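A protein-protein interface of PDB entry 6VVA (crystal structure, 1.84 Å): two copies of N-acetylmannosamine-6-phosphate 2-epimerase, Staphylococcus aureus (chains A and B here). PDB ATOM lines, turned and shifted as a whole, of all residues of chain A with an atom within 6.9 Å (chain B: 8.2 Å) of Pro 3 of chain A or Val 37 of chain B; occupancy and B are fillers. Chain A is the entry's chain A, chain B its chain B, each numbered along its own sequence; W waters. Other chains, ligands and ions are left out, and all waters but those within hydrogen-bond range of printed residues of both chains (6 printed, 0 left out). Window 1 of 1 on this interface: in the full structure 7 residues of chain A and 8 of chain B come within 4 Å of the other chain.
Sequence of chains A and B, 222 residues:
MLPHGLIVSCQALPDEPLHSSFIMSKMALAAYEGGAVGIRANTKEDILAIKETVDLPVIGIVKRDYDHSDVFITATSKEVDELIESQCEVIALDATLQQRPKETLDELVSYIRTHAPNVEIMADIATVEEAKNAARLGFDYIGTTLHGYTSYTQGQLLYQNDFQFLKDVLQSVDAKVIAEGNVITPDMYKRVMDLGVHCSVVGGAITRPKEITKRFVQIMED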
ATOM      1  N   MET A   1       3.147  20.197  19.851  1.00  0.00           N
ATOM      2  CA  MET A   1       2.331  21.430  19.666  1.00  0.00           C
ATOM      3  C   MET A   1       1.418  21.627  20.882  1.00  0.00           C
ATOM      4  O   MET A   1       1.126  20.628  21.569  1.00  0.00           O
ATOM      5  CB  MET A   1       1.467  21.333  18.405  1.00  0.00           C
ATOM      6  CG  MET A   1       2.263  21.390  17.119  1.00  0.00           C
ATOM      7  SD  MET A   1       1.204  21.530  15.658  1.00  0.00           S
ATOM      8  CE  MET A   1       2.436  21.464  14.359  1.00  0.00           C
ATOM      9  N   LEU A   2       0.995  22.870  21.132  1.00  0.00           N
ATOM     10  CA  LEU A   2      -0.026  23.201  22.162  1.00  0.00           C
ATOM     11  C   LEU A   2      -1.388  22.741  21.654  1.00  0.00           C
ATOM     12  O   LEU A   2      -1.764  23.063  20.530  1.00  0.00           O
ATOM     13  CB  LEU A   2      -0.025  24.710  22.434  1.00  0.00           C
ATOM     14  CG  LEU A   2       1.261  25.280  23.031  1.00  0.00           C
ATOM     15  CD1 LEU A   2       1.174  26.793  23.143  1.00  0.00           C
ATOM     16  CD2 LEU A   2       1.560  24.662  24.390  1.00  0.00           C
ATOM     17  N   PRO A   3      -2.155  21.948  22.436  1.00  0.00           N
ATOM     18  CA  PRO A   3      -3.539  21.639  22.080  1.00  0.00           C
ATOM     19  C   PRO A   3      -4.420  22.896  22.119  1.00  0.00           C
ATOM     20  O   PRO A   3      -3.985  23.908  22.647  1.00  0.00           O
ATOM     21  CB  PRO A   3      -4.000  20.640  23.155  1.00  0.00           C
ATOM     22  CG  PRO A   3      -2.720  20.126  23.781  1.00  0.00           C
ATOM     23  CD  PRO A   3      -1.732  21.269  23.671  1.00  0.00           C
ATOM     24  N   HIS A   4      -5.628  22.806  21.559  1.00  0.00           N
ATOM     25  CA  HIS A   4      -6.729  23.774  21.805  1.00  0.00           C
ATOM     26  C   HIS A   4      -7.135  23.655  23.277  1.00  0.00           C
ATOM     27  O   HIS A   4      -7.117  22.522  23.793  1.00  0.00           O
ATOM     28  CB  HIS A   4      -7.920  23.516  20.871  1.00  0.00           C
ATOM     29  CG  HIS A   4      -7.648  23.805  19.435  1.00  0.00           C
ATOM     30  ND1 HIS A   4      -7.930  25.028  18.860  1.00  0.00           N
ATOM     31  CD2 HIS A   4      -7.136  23.035  18.450  1.00  0.00           C
ATOM     32  CE1 HIS A   4      -7.600  25.001  17.584  1.00  0.00           C
ATOM     33  NE2 HIS A   4      -7.112  23.789  17.307  1.00  0.00           N
ATOM     34  N   GLY A   5      -7.457  24.772  23.930  1.00  0.00           N
ATOM     35  CA  GLY A   5      -8.042  24.771  25.285  1.00  0.00           C
ATOM     36  C   GLY A   5      -7.373  25.767  26.211  1.00  0.00           C
ATOM     37  O   GLY A   5      -6.925  26.824  25.729  1.00  0.00           O
ATOM     38  N   LEU A   6      -7.323  25.438  27.504  1.00  0.00           N
ATOM     39  CA  LEU A   6      -6.925  26.369  28.591  1.00  0.00           C
ATOM     40  C   LEU A   6      -5.457  26.147  28.969  1.00  0.00           C
ATOM     41  O   LEU A   6      -5.093  25.019  29.354  1.00  0.00           O
ATOM     42  CB  LEU A   6      -7.838  26.142  29.801  1.00  0.00           C
ATOM     43  CG  LEU A   6      -7.584  27.059  30.998  1.00  0.00           C
ATOM     44  CD1 LEU A   6      -7.888  28.509  30.652  1.00  0.00           C
ATOM     45  CD2 LEU A   6      -8.403  26.614  32.198  1.00  0.00           C
ATOM     46  N   ILE A   7      -4.650  27.206  28.849  1.00  0.00           N
ATOM     47  CA  ILE A   7      -3.262  27.303  29.391  1.00  0.00           C
ATOM     48  C   ILE A   7      -3.332  28.096  30.699  1.00  0.00           C
ATOM     49  O   ILE A   7      -3.888  29.211  30.675  1.00  0.00           O
ATOM     50  CB  ILE A   7      -2.320  27.976  28.372  1.00  0.00           C
ATOM     51  CG1 ILE A   7      -2.471  27.381  26.971  1.00  0.00           C
ATOM     52  CG2 ILE A   7      -0.880  27.926  28.858  1.00  0.00           C
ATOM     53  CD1 ILE A   7      -1.981  25.958  26.848  1.00  0.00           C
ATOM     54  N   VAL A  37      -4.469  22.221  29.460  1.00  0.00           N
ATOM     55  CA  VAL A  37      -3.731  21.527  28.359  1.00  0.00           C
ATOM     56  C   VAL A  37      -2.286  22.041  28.304  1.00  0.00           C
ATOM     57  O   VAL A  37      -1.500  21.480  27.521  1.00  0.00           O
ATOM     58  CB  VAL A  37      -4.438  21.681  26.997  1.00  0.00           C
ATOM     59  CG1 VAL A  37      -5.841  21.098  27.029  1.00  0.00           C
ATOM     60  CG2 VAL A  37      -4.467  23.122  26.502  1.00  0.00           C
ATOM     61  N   GLY A  38      -1.947  23.066  29.092  1.00  0.00           N
ATOM     62  CA  GLY A  38      -0.582  23.619  29.145  1.00  0.00           C
ATOM     63  C   GLY A  38      -0.373  24.541  30.330  1.00  0.00           C
ATOM     64  O   GLY A  38      -1.363  24.886  31.009  1.00  0.00           O
ATOM     65  N   PRO A  57       2.778  20.635  28.298  1.00  0.00           N
ATOM     66  CA  PRO A  57       3.701  21.522  27.596  1.00  0.00           C
ATOM     67  C   PRO A  57       3.769  22.865  28.335  1.00  0.00           C
ATOM     68  O   PRO A  57       2.743  23.325  28.818  1.00  0.00           O
ATOM     69  CB  PRO A  57       3.109  21.643  26.184  1.00  0.00           C
ATOM     70  CG  PRO A  57       1.640  21.319  26.365  1.00  0.00           C
ATOM     71  CD  PRO A  57       1.591  20.308  27.493  1.00  0.00           C
ATOM     72  N   TYR A 141       3.195  30.861  17.690  1.00  0.00           N
ATOM     73  CA  TYR A 141       2.059  31.428  18.464  1.00  0.00           C
ATOM     74  C   TYR A 141       2.240  32.941  18.607  1.00  0.00           C
ATOM     75  O   TYR A 141       3.387  33.405  18.756  1.00  0.00           O
ATOM     76  CB  TYR A 141       1.948  30.754  19.833  1.00  0.00           C
ATOM     77  CG  TYR A 141       1.954  29.248  19.777  1.00  0.00           C
ATOM     78  CD1 TYR A 141       0.798  28.538  19.498  1.00  0.00           C
ATOM     79  CD2 TYR A 141       3.123  28.531  19.978  1.00  0.00           C
ATOM     80  CE1 TYR A 141       0.798  27.154  19.432  1.00  0.00           C
ATOM     81  CE2 TYR A 141       3.140  27.146  19.919  1.00  0.00           C
ATOM     82  CZ  TYR A 141       1.973  26.455  19.643  1.00  0.00           C
ATOM     83  OH  TYR A 141       1.976  25.092  19.575  1.00  0.00           O
ATOM     84  N   HIS A 198      -6.486  29.900  19.122  1.00  0.00           N
ATOM     85  CA  HIS A 198      -6.004  28.499  19.230  1.00  0.00           C
ATOM     86  C   HIS A 198      -6.211  28.014  20.669  1.00  0.00           C
ATOM     87  O   HIS A 198      -6.810  26.944  20.859  1.00  0.00           O
ATOM     88  CB  HIS A 198      -4.542  28.381  18.790  1.00  0.00           C
ATOM     89  CG  HIS A 198      -4.038  26.982  18.879  1.00  0.00           C
ATOM     90  ND1 HIS A 198      -4.339  26.033  17.925  1.00  0.00           N
ATOM     91  CD2 HIS A 198      -3.302  26.357  19.823  1.00  0.00           C
ATOM     92  CE1 HIS A 198      -3.791  24.885  18.266  1.00  0.00           C
ATOM     93  NE2 HIS A 198      -3.150  25.059  19.428  1.00  0.00           N
ATOM     94  N   CYS A 199      -5.731  28.791  21.639  1.00  0.00           N
ATOM     95  CA  CYS A 199      -5.925  28.557  23.092  1.00  0.00           C
ATOM     96  C   CYS A 199      -5.919  29.905  23.818  1.00  0.00           C
ATOM     97  O   CYS A 199      -5.658  30.938  23.170  1.00  0.00           O
ATOM     98  CB  CYS A 199      -4.858  27.619  23.647  1.00  0.00           C
ATOM     99  SG  CYS A 199      -3.164  28.123  23.257  1.00  0.00           S
ATOM    100  N   SER A 200      -6.172  29.843  25.128  1.00  0.00           N
ATOM    101  CA  SER A 200      -6.187  31.059  25.971  1.00  0.00           C
ATOM    102  C   SER A 200      -5.363  30.846  27.246  1.00  0.00           C
ATOM    103  O   SER A 200      -5.287  29.701  27.686  1.00  0.00           O
ATOM    104  CB  SER A 200      -7.595  31.480  26.311  1.00  0.00           C
ATOM    105  OG  SER A 200      -7.595  32.609  27.166  1.00  0.00           O
ATOM    106  N   MET B   1      -5.281  15.028  32.196  1.00  0.00           N
ATOM    107  CA  MET B   1      -6.368  14.452  31.350  1.00  0.00           C
ATOM    108  C   MET B   1      -6.008  14.612  29.869  1.00  0.00           C
ATOM    109  O   MET B   1      -5.199  15.505  29.547  1.00  0.00           O
ATOM    110  CB  MET B   1      -7.704  15.150  31.622  1.00  0.00           C
ATOM    111  CG  MET B   1      -8.163  15.033  33.062  1.00  0.00           C
ATOM    112  SD  MET B   1      -9.903  15.488  33.274  1.00  0.00           S
ATOM    113  CE  MET B   1      -9.812  17.260  33.047  1.00  0.00           C
ATOM    114  N   LEU B   2      -6.588  13.773  29.004  1.00  0.00           N
ATOM    115  CA  LEU B   2      -6.405  13.845  27.529  1.00  0.00           C
ATOM    116  C   LEU B   2      -7.036  15.140  27.027  1.00  0.00           C
ATOM    117  O   LEU B   2      -8.179  15.438  27.363  1.00  0.00           O
ATOM    118  CB  LEU B   2      -7.059  12.631  26.861  1.00  0.00           C
ATOM    119  CG  LEU B   2      -6.461  11.268  27.208  1.00  0.00           C
ATOM    120  CD1 LEU B   2      -7.292  10.148  26.601  1.00  0.00           C
ATOM    121  CD2 LEU B   2      -5.016  11.166  26.748  1.00  0.00           C
ATOM    122  N   PRO B   3      -6.316  15.964  26.230  1.00  0.00           N
ATOM    123  CA  PRO B   3      -6.933  17.109  25.565  1.00  0.00           C
ATOM    124  C   PRO B   3      -7.913  16.658  24.473  1.00  0.00           C
ATOM    125  O   PRO B   3      -7.900  15.493  24.111  1.00  0.00           O
ATOM    126  CB  PRO B   3      -5.763  17.867  24.918  1.00  0.00           C
ATOM    127  CG  PRO B   3      -4.519  17.299  25.573  1.00  0.00           C
ATOM    128  CD  PRO B   3      -4.874  15.879  25.960  1.00  0.00           C
ATOM    129  N   HIS B   4      -8.727  17.590  23.973  1.00  0.00           N
ATOM    130  CA  HIS B   4      -9.480  17.440  22.700  1.00  0.00           C
ATOM    131  C   HIS B   4      -8.466  17.335  21.558  1.00  0.00           C
ATOM    132  O   HIS B   4      -7.394  17.967  21.666  1.00  0.00           O
ATOM    133  CB  HIS B   4     -10.446  18.612  22.481  1.00  0.00           C
ATOM    134  CG  HIS B   4     -11.599  18.634  23.426  1.00  0.00           C
ATOM    135  ND1 HIS B   4     -12.813  18.056  23.118  1.00  0.00           N
ATOM    136  CD2 HIS B   4     -11.735  19.166  24.659  1.00  0.00           C
ATOM    137  CE1 HIS B   4     -13.648  18.229  24.122  1.00  0.00           C
ATOM    138  NE2 HIS B   4     -13.010  18.907  25.081  1.00  0.00           N
ATOM    139  N   GLY B   5      -8.784  16.557  20.520  1.00  0.00           N
ATOM    140  CA  GLY B   5      -7.998  16.497  19.273  1.00  0.00           C
ATOM    141  C   GLY B   5      -7.643  15.078  18.873  1.00  0.00           C
ATOM    142  O   GLY B   5      -8.428  14.154  19.170  1.00  0.00           O
ATOM    143  N   LEU B   6      -6.495  14.919  18.210  1.00  0.00           N
ATOM    144  CA  LEU B   6      -6.090  13.668  17.521  1.00  0.00           C
ATOM    145  C   LEU B   6      -5.135  12.870  18.410  1.00  0.00           C
ATOM    146  O   LEU B   6      -4.073  13.410  18.788  1.00  0.00           O
ATOM    147  CB  LEU B   6      -5.428  14.024  16.187  1.00  0.00           C
ATOM    148  CG  LEU B   6      -4.980  12.836  15.338  1.00  0.00           C
ATOM    149  CD1 LEU B   6      -6.174  12.049  14.823  1.00  0.00           C
ATOM    150  CD2 LEU B   6      -4.109  13.299  14.183  1.00  0.00           C
ATOM    151  N   ILE B   7      -5.527  11.636  18.733  1.00  0.00           N
ATOM    152  CA  ILE B   7      -4.647  10.627  19.392  1.00  0.00           C
ATOM    153  C   ILE B   7      -4.160   9.663  18.305  1.00  0.00           C
ATOM    154  O   ILE B   7      -5.011   9.120  17.579  1.00  0.00           O
ATOM    155  CB  ILE B   7      -5.389   9.905  20.535  1.00  0.00           C
ATOM    156  CG1 ILE B   7      -5.855  10.894  21.608  1.00  0.00           C
ATOM    157  CG2 ILE B   7      -4.537   8.794  21.129  1.00  0.00           C
ATOM    158  CD1 ILE B   7      -6.391  10.237  22.855  1.00  0.00           C
ATOM    159  N   VAL B   8      -2.843   9.491  18.189  1.00  0.00           N
ATOM    160  CA  VAL B   8      -2.228   8.594  17.167  1.00  0.00           C
ATOM    161  C   VAL B   8      -1.843   7.279  17.850  1.00  0.00           C
ATOM    162  O   VAL B   8      -1.037   7.314  18.798  1.00  0.00           O
ATOM    163  CB  VAL B   8      -1.035   9.263  16.458  1.00  0.00           C
ATOM    164  CG1 VAL B   8      -0.374   8.327  15.455  1.00  0.00           C
ATOM    165  CG2 VAL B   8      -1.457  10.554  15.775  1.00  0.00           C
ATOM    166  N   ALA B  31       4.068  11.772  15.095  1.00  0.00           N
ATOM    167  CA  ALA B  31       2.690  12.152  15.492  1.00  0.00           C
ATOM    168  C   ALA B  31       2.726  13.468  16.278  1.00  0.00           C
ATOM    169  O   ALA B  31       1.925  14.366  15.969  1.00  0.00           O
ATOM    170  CB  ALA B  31       2.060  11.046  16.301  1.00  0.00           C
ATOM    171  N   TYR B  32       3.633  13.573  17.253  1.00  0.00           N
ATOM    172  CA  TYR B  32       3.839  14.785  18.091  1.00  0.00           C
ATOM    173  C   TYR B  32       4.147  15.988  17.191  1.00  0.00           C
ATOM    174  O   TYR B  32       3.490  17.033  17.339  1.00  0.00           O
ATOM    175  CB  TYR B  32       4.950  14.543  19.116  1.00  0.00           C
ATOM    176  CG  TYR B  32       5.333  15.758  19.922  1.00  0.00           C
ATOM    177  CD1 TYR B  32       4.427  16.355  20.784  1.00  0.00           C
ATOM    178  CD2 TYR B  32       6.601  16.310  19.831  1.00  0.00           C
ATOM    179  CE1 TYR B  32       4.768  17.471  21.532  1.00  0.00           C
ATOM    180  CE2 TYR B  32       6.958  17.424  20.572  1.00  0.00           C
ATOM    181  CZ  TYR B  32       6.039  18.006  21.428  1.00  0.00           C
ATOM    182  OH  TYR B  32       6.377  19.105  22.164  1.00  0.00           O
ATOM    183  N   GLY B  34       3.496  16.378  14.121  1.00  0.00           N
ATOM    184  CA  GLY B  34       2.338  16.593  13.230  1.00  0.00           C
ATOM    185  C   GLY B  34       1.166  17.275  13.924  1.00  0.00           C
ATOM    186  O   GLY B  34       0.266  17.755  13.205  1.00  0.00           O
ATOM    187  N   GLY B  35       1.151  17.299  15.263  1.00  0.00           N
ATOM    188  CA  GLY B  35       0.145  18.022  16.067  1.00  0.00           C
ATOM    189  C   GLY B  35      -0.805  17.104  16.824  1.00  0.00           C
ATOM    190  O   GLY B  35      -1.885  17.586  17.219  1.00  0.00           O
ATOM    191  N   ALA B  36      -0.428  15.839  17.047  1.00  0.00           N
ATOM    192  CA  ALA B  36      -1.170  14.889  17.909  1.00  0.00           C
ATOM    193  C   ALA B  36      -1.169  15.414  19.349  1.00  0.00           C
ATOM    194  O   ALA B  36      -0.177  16.057  19.745  1.00  0.00           O
ATOM    195  CB  ALA B  36      -0.552  13.514  17.826  1.00  0.00           C
ATOM    196  N   VAL B  37      -2.244  15.154  20.100  1.00  0.00           N
ATOM    197  CA  VAL B  37      -2.403  15.594  21.520  1.00  0.00           C
ATOM    198  C   VAL B  37      -2.166  14.401  22.454  1.00  0.00           C
ATOM    199  O   VAL B  37      -2.135  14.617  23.677  1.00  0.00           O
ATOM    200  CB  VAL B  37      -3.778  16.242  21.772  1.00  0.00           C
ATOM    201  CG1 VAL B  37      -3.993  17.453  20.880  1.00  0.00           C
ATOM    202  CG2 VAL B  37      -4.929  15.255  21.623  1.00  0.00           C
ATOM    203  N   GLY B  38      -2.004  13.195  21.904  1.00  0.00           N
ATOM    204  CA  GLY B  38      -1.763  11.977  22.696  1.00  0.00           C
ATOM    205  C   GLY B  38      -1.345  10.803  21.834  1.00  0.00           C
ATOM    206  O   GLY B  38      -1.421  10.909  20.593  1.00  0.00           O
ATOM    207  N   ILE B  39      -0.922   9.718  22.482  1.00  0.00           N
ATOM    208  CA  ILE B  39      -0.460   8.459  21.833  1.00  0.00           C
ATOM    209  C   ILE B  39      -1.212   7.291  22.474  1.00  0.00           C
ATOM    210  O   ILE B  39      -1.402   7.311  23.703  1.00  0.00           O
ATOM    211  CB  ILE B  39       1.068   8.297  21.974  1.00  0.00           C
ATOM    212  CG1 ILE B  39       1.833   9.494  21.404  1.00  0.00           C
ATOM    213  CG2 ILE B  39       1.534   6.983  21.359  1.00  0.00           C
ATOM    214  CD1 ILE B  39       1.715   9.660  19.904  1.00  0.00           C
ATOM    215  N   ARG B  40      -1.630   6.320  21.663  1.00  0.00           N
ATOM    216  CA  ARG B  40      -2.048   4.975  22.129  1.00  0.00           C
ATOM    217  C   ARG B  40      -0.936   3.994  21.741  1.00  0.00           C
ATOM    218  O   ARG B  40      -0.500   4.037  20.574  1.00  0.00           O
ATOM    219  CB  ARG B  40      -3.412   4.607  21.542  1.00  0.00           C
ATOM    220  CG  ARG B  40      -3.864   3.193  21.875  1.00  0.00           C
ATOM    221  CD  ARG B  40      -5.370   3.082  21.999  1.00  0.00           C
ATOM    222  NE  ARG B  40      -5.802   1.691  22.029  1.00  0.00           N
ATOM    223  CZ  ARG B  40      -6.879   1.230  22.665  1.00  0.00           C
ATOM    224  NH1 ARG B  40      -7.659   2.044  23.359  1.00  0.00           N
ATOM    225  NH2 ARG B  40      -7.165  -0.060  22.609  1.00  0.00           N
ATOM    226  N   ASP B  55       6.486  13.755  25.573  1.00  0.00           N
ATOM    227  CA  ASP B  55       5.823  13.976  26.886  1.00  0.00           C
ATOM    228  C   ASP B  55       4.298  13.941  26.715  1.00  0.00           C
ATOM    229  O   ASP B  55       3.597  14.168  27.725  1.00  0.00           O
ATOM    230  CB  ASP B  55       6.293  15.287  27.523  1.00  0.00           C
ATOM    231  CG  ASP B  55       7.711  15.226  28.069  1.00  0.00           C
ATOM    232  OD1 ASP B  55       8.122  14.135  28.517  1.00  0.00           O
ATOM    233  OD2 ASP B  55       8.391  16.267  28.042  1.00  0.00           O
ATOM    234  N   LEU B  56       3.806  13.653  25.501  1.00  0.00           N
ATOM    235  CA  LEU B  56       2.358  13.476  25.208  1.00  0.00           C
ATOM    236  C   LEU B  56       1.787  12.421  26.151  1.00  0.00           C
ATOM    237  O   LEU B  56       2.458  11.435  26.457  1.00  0.00           O
ATOM    238  CB  LEU B  56       2.161  13.039  23.752  1.00  0.00           C
ATOM    239  CG  LEU B  56       2.410  14.099  22.680  1.00  0.00           C
ATOM    240  CD1 LEU B  56       2.181  13.511  21.295  1.00  0.00           C
ATOM    241  CD2 LEU B  56       1.525  15.320  22.893  1.00  0.00           C
ATOM    242  N   PRO B  57       0.528  12.577  26.621  1.00  0.00           N
ATOM    243  CA  PRO B  57      -0.117  11.539  27.422  1.00  0.00           C
ATOM    244  C   PRO B  57      -0.253  10.262  26.584  1.00  0.00           C
ATOM    245  O   PRO B  57      -0.479  10.367  25.387  1.00  0.00           O
ATOM    246  CB  PRO B  57      -1.480  12.139  27.799  1.00  0.00           C
ATOM    247  CG  PRO B  57      -1.727  13.200  26.746  1.00  0.00           C
ATOM    248  CD  PRO B  57      -0.354  13.730  26.385  1.00  0.00           C
ATOM    249  N   VAL B  58      -0.081   9.101  27.218  1.00  0.00           N
ATOM    250  CA  VAL B  58      -0.115   7.771  26.544  1.00  0.00           C
ATOM    251  C   VAL B  58      -1.290   6.965  27.101  1.00  0.00           C
ATOM    252  O   VAL B  58      -1.380   6.819  28.339  1.00  0.00           O
ATOM    253  CB  VAL B  58       1.220   7.019  26.705  1.00  0.00           C
ATOM    254  CG1 VAL B  58       1.171   5.632  26.080  1.00  0.00           C
ATOM    255  CG2 VAL B  58       2.380   7.821  26.134  1.00  0.00           C
ATOM    256  N   TYR B 189     -12.486  11.788  10.628  1.00  0.00           N
ATOM    257  CA  TYR B 189     -11.970  12.440  11.859  1.00  0.00           C
ATOM    258  C   TYR B 189     -12.789  13.706  12.142  1.00  0.00           C
ATOM    259  O   TYR B 189     -13.243  13.877  13.285  1.00  0.00           O
ATOM    260  CB  TYR B 189     -10.471  12.736  11.747  1.00  0.00           C
ATOM    261  CG  TYR B 189      -9.922  13.570  12.876  1.00  0.00           C
ATOM    262  CD1 TYR B 189     -10.225  13.270  14.196  1.00  0.00           C
ATOM    263  CD2 TYR B 189      -9.103  14.660  12.632  1.00  0.00           C
ATOM    264  CE1 TYR B 189      -9.736  14.035  15.241  1.00  0.00           C
ATOM    265  CE2 TYR B 189      -8.604  15.435  13.667  1.00  0.00           C
ATOM    266  CZ  TYR B 189      -8.919  15.119  14.977  1.00  0.00           C
ATOM    267  OH  TYR B 189      -8.440  15.874  16.005  1.00  0.00           O
ATOM    268  N   MET B 193     -15.583  14.309  15.459  1.00  0.00           N
ATOM    269  CA  MET B 193     -15.287  15.492  16.314  1.00  0.00           C
ATOM    270  C   MET B 193     -16.487  16.450  16.296  1.00  0.00           C
ATOM    271  O   MET B 193     -16.855  16.942  17.376  1.00  0.00           O
ATOM    272  CB  MET B 193     -14.025  16.223  15.844  1.00  0.00           C
ATOM    273  CG  MET B 193     -12.752  15.412  16.029  1.00  0.00           C
ATOM    274  SD  MET B 193     -12.410  14.990  17.759  1.00  0.00           S
ATOM    275  CE  MET B 193     -11.907  16.588  18.393  1.00  0.00           C
ATOM    276  N   HIS B 198     -14.848  13.497  22.653  1.00  0.00           N
ATOM    277  CA  HIS B 198     -13.774  14.231  23.372  1.00  0.00           C
ATOM    278  C   HIS B 198     -12.533  14.291  22.475  1.00  0.00           C
ATOM    279  O   HIS B 198     -12.002  15.395  22.263  1.00  0.00           O
ATOM    280  CB  HIS B 198     -13.470  13.580  24.726  1.00  0.00           C
ATOM    281  CG  HIS B 198     -12.460  14.339  25.513  1.00  0.00           C
ATOM    282  ND1 HIS B 198     -12.788  15.474  26.228  1.00  0.00           N
ATOM    283  CD2 HIS B 198     -11.131  14.159  25.671  1.00  0.00           C
ATOM    284  CE1 HIS B 198     -11.705  15.949  26.810  1.00  0.00           C
ATOM    285  NE2 HIS B 198     -10.676  15.162  26.483  1.00  0.00           N
ATOM    286  N   CYS B 199     -12.105  13.137  21.963  1.00  0.00           N
ATOM    287  CA  CYS B 199     -10.978  12.997  21.005  1.00  0.00           C
ATOM    288  C   CYS B 199     -11.218  11.765  20.128  1.00  0.00           C
ATOM    289  O   CYS B 199     -12.218  11.051  20.348  1.00  0.00           O
ATOM    290  CB  CYS B 199      -9.646  12.920  21.746  1.00  0.00           C
ATOM    291  SG  CYS B 199      -9.582  11.617  23.001  1.00  0.00           S
ATOM    292  N   SER B 200     -10.306  11.557  19.173  1.00  0.00           N
ATOM    293  CA  SER B 200     -10.386  10.394  18.257  1.00  0.00           C
ATOM    294  C   SER B 200      -9.013   9.713  18.138  1.00  0.00           C
ATOM    295  O   SER B 200      -8.012  10.421  18.211  1.00  0.00           O
ATOM    296  CB  SER B 200     -10.901  10.788  16.896  1.00  0.00           C
ATOM    297  OG  SER B 200     -11.838  11.846  16.984  1.00  0.00           O
HETATM  298  O   HOH W   1      -0.356  18.404  21.775  1.00  0.00           O
HETATM  299  O   HOH W   2       1.606  17.930  19.084  1.00  0.00           O
HETATM  300  O   HOH W   3       4.225  20.772  22.681  1.00  0.00           O
HETATM  301  O   HOH W   4      -0.286  20.289  12.420  1.00  0.00           O
HETATM  302  O   HOH W   5      -8.516  20.467  24.590  1.00  0.00           O
HETATM  303  O   HOH W   6      -6.741  20.278  20.482  1.00  0.00           O
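Hydrophobic or aromatic side chains of chain B that line the printed part of chain A: Pro 3, Tyr 32 and Val 37.
Of the 14 printed residues of chain A, 3 touch a printed residue of chain B.
Hydrophobic or aromatic side chains of chain A that line the printed part of chain B: Met 1, Pro 3 and Val 37.
Among the printed residues, 5 pairs touch across the chains.
The backbone carbonyl oxygen (O) of Leu 6 of chain A sits at hydrogen-bond distance from the backbone NH (N) of Val 37 of chain A, 2.9 Å away.
The backbone carbonyl oxygen (O) of Leu 6 of chain B sits at hydrogen-bond distance from the backbone NH (N) of Val 37 of chain B, 2.8 Å away.
Pro 3 of chain B touches its own counterpart, Pro 3 of chain A.
Pro 3 of chain A touches Val 37 of chain B, and with the chains exchanged Val 37 of chain A touches Pro 3 of chain B.
Positions printed for both chains: 1, 2, 3, 4, 5, 6, 7, 37, 38, 57, 198, 199 and 200.
Pro 57 of chain A touches none of the printed residues of chain B.
Of the printed residues of chain A, Pro 3 of chain B touches Pro 3 and Val 37.
Of the printed residues of chain A, Gly 35 of chain B touches Met 1 (3.7 Å).
Val 37 of chain B touches one residue of chain A.
The nearest residue of chain B that does not touch Pro 3 of chain A is His 4 of chain B (4.6 Å).
The nearest residue of chain A that does not touch Val 37 of chain B is His 4 of chain A (5.6 Å).
The nearest printed residue of chain A that does not touch Tyr 32 of chain B is Pro 57 of chain A (5.8 Å).
Water W5 bridges the backbone carbonyl oxygen of His 4 of chain A (2.6 Å) and the backbone NH of His 4 of chain B (2.9 Å).
Water W2 lies within hydrogen-bond range of the backbone carbonyl oxygen (O) of Ala 36 of chain B (2.7 Å), the backbone carbonyl oxygen (O) of Tyr 32 of chain B (2.7 Å) and the backbone NH (N) of Met 1 of chain A (2.8 Å).
Water W6 bridges the backbone carbonyl oxygen of His 4 of chain B (2.7 Å) and the backbone NH of His 4 of chain A (3.0 Å).
Water W1 bridges O of Met 1 of chain A (2.7 Å) and O of Ala 36 of chain B (3.1 Å).
Water W4 lies within hydrogen-bond range of O of Gly 34 of chain B (2.7 Å) and SD of Met 1 of chain A (3.8 Å).
Water W3 bridges OH of Tyr 32 of chain B (2.8 Å) and N of Met 1 of chain A (3.1 Å).
Among the printed residues, merely in contact across the chains: Met 1 of chain A with Tyr 32 of chain B (3.6 Å), Met 1 of chain A with Gly 35 of chain B (3.7 Å), Pro 3 of chain A with Pro 3 of chain B (3.7 Å), Pro 3 of chain A with Val 37 of chain B (3.9 Å) and Val 37 of chain A with Pro 3 of chain B (3.9 Å).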
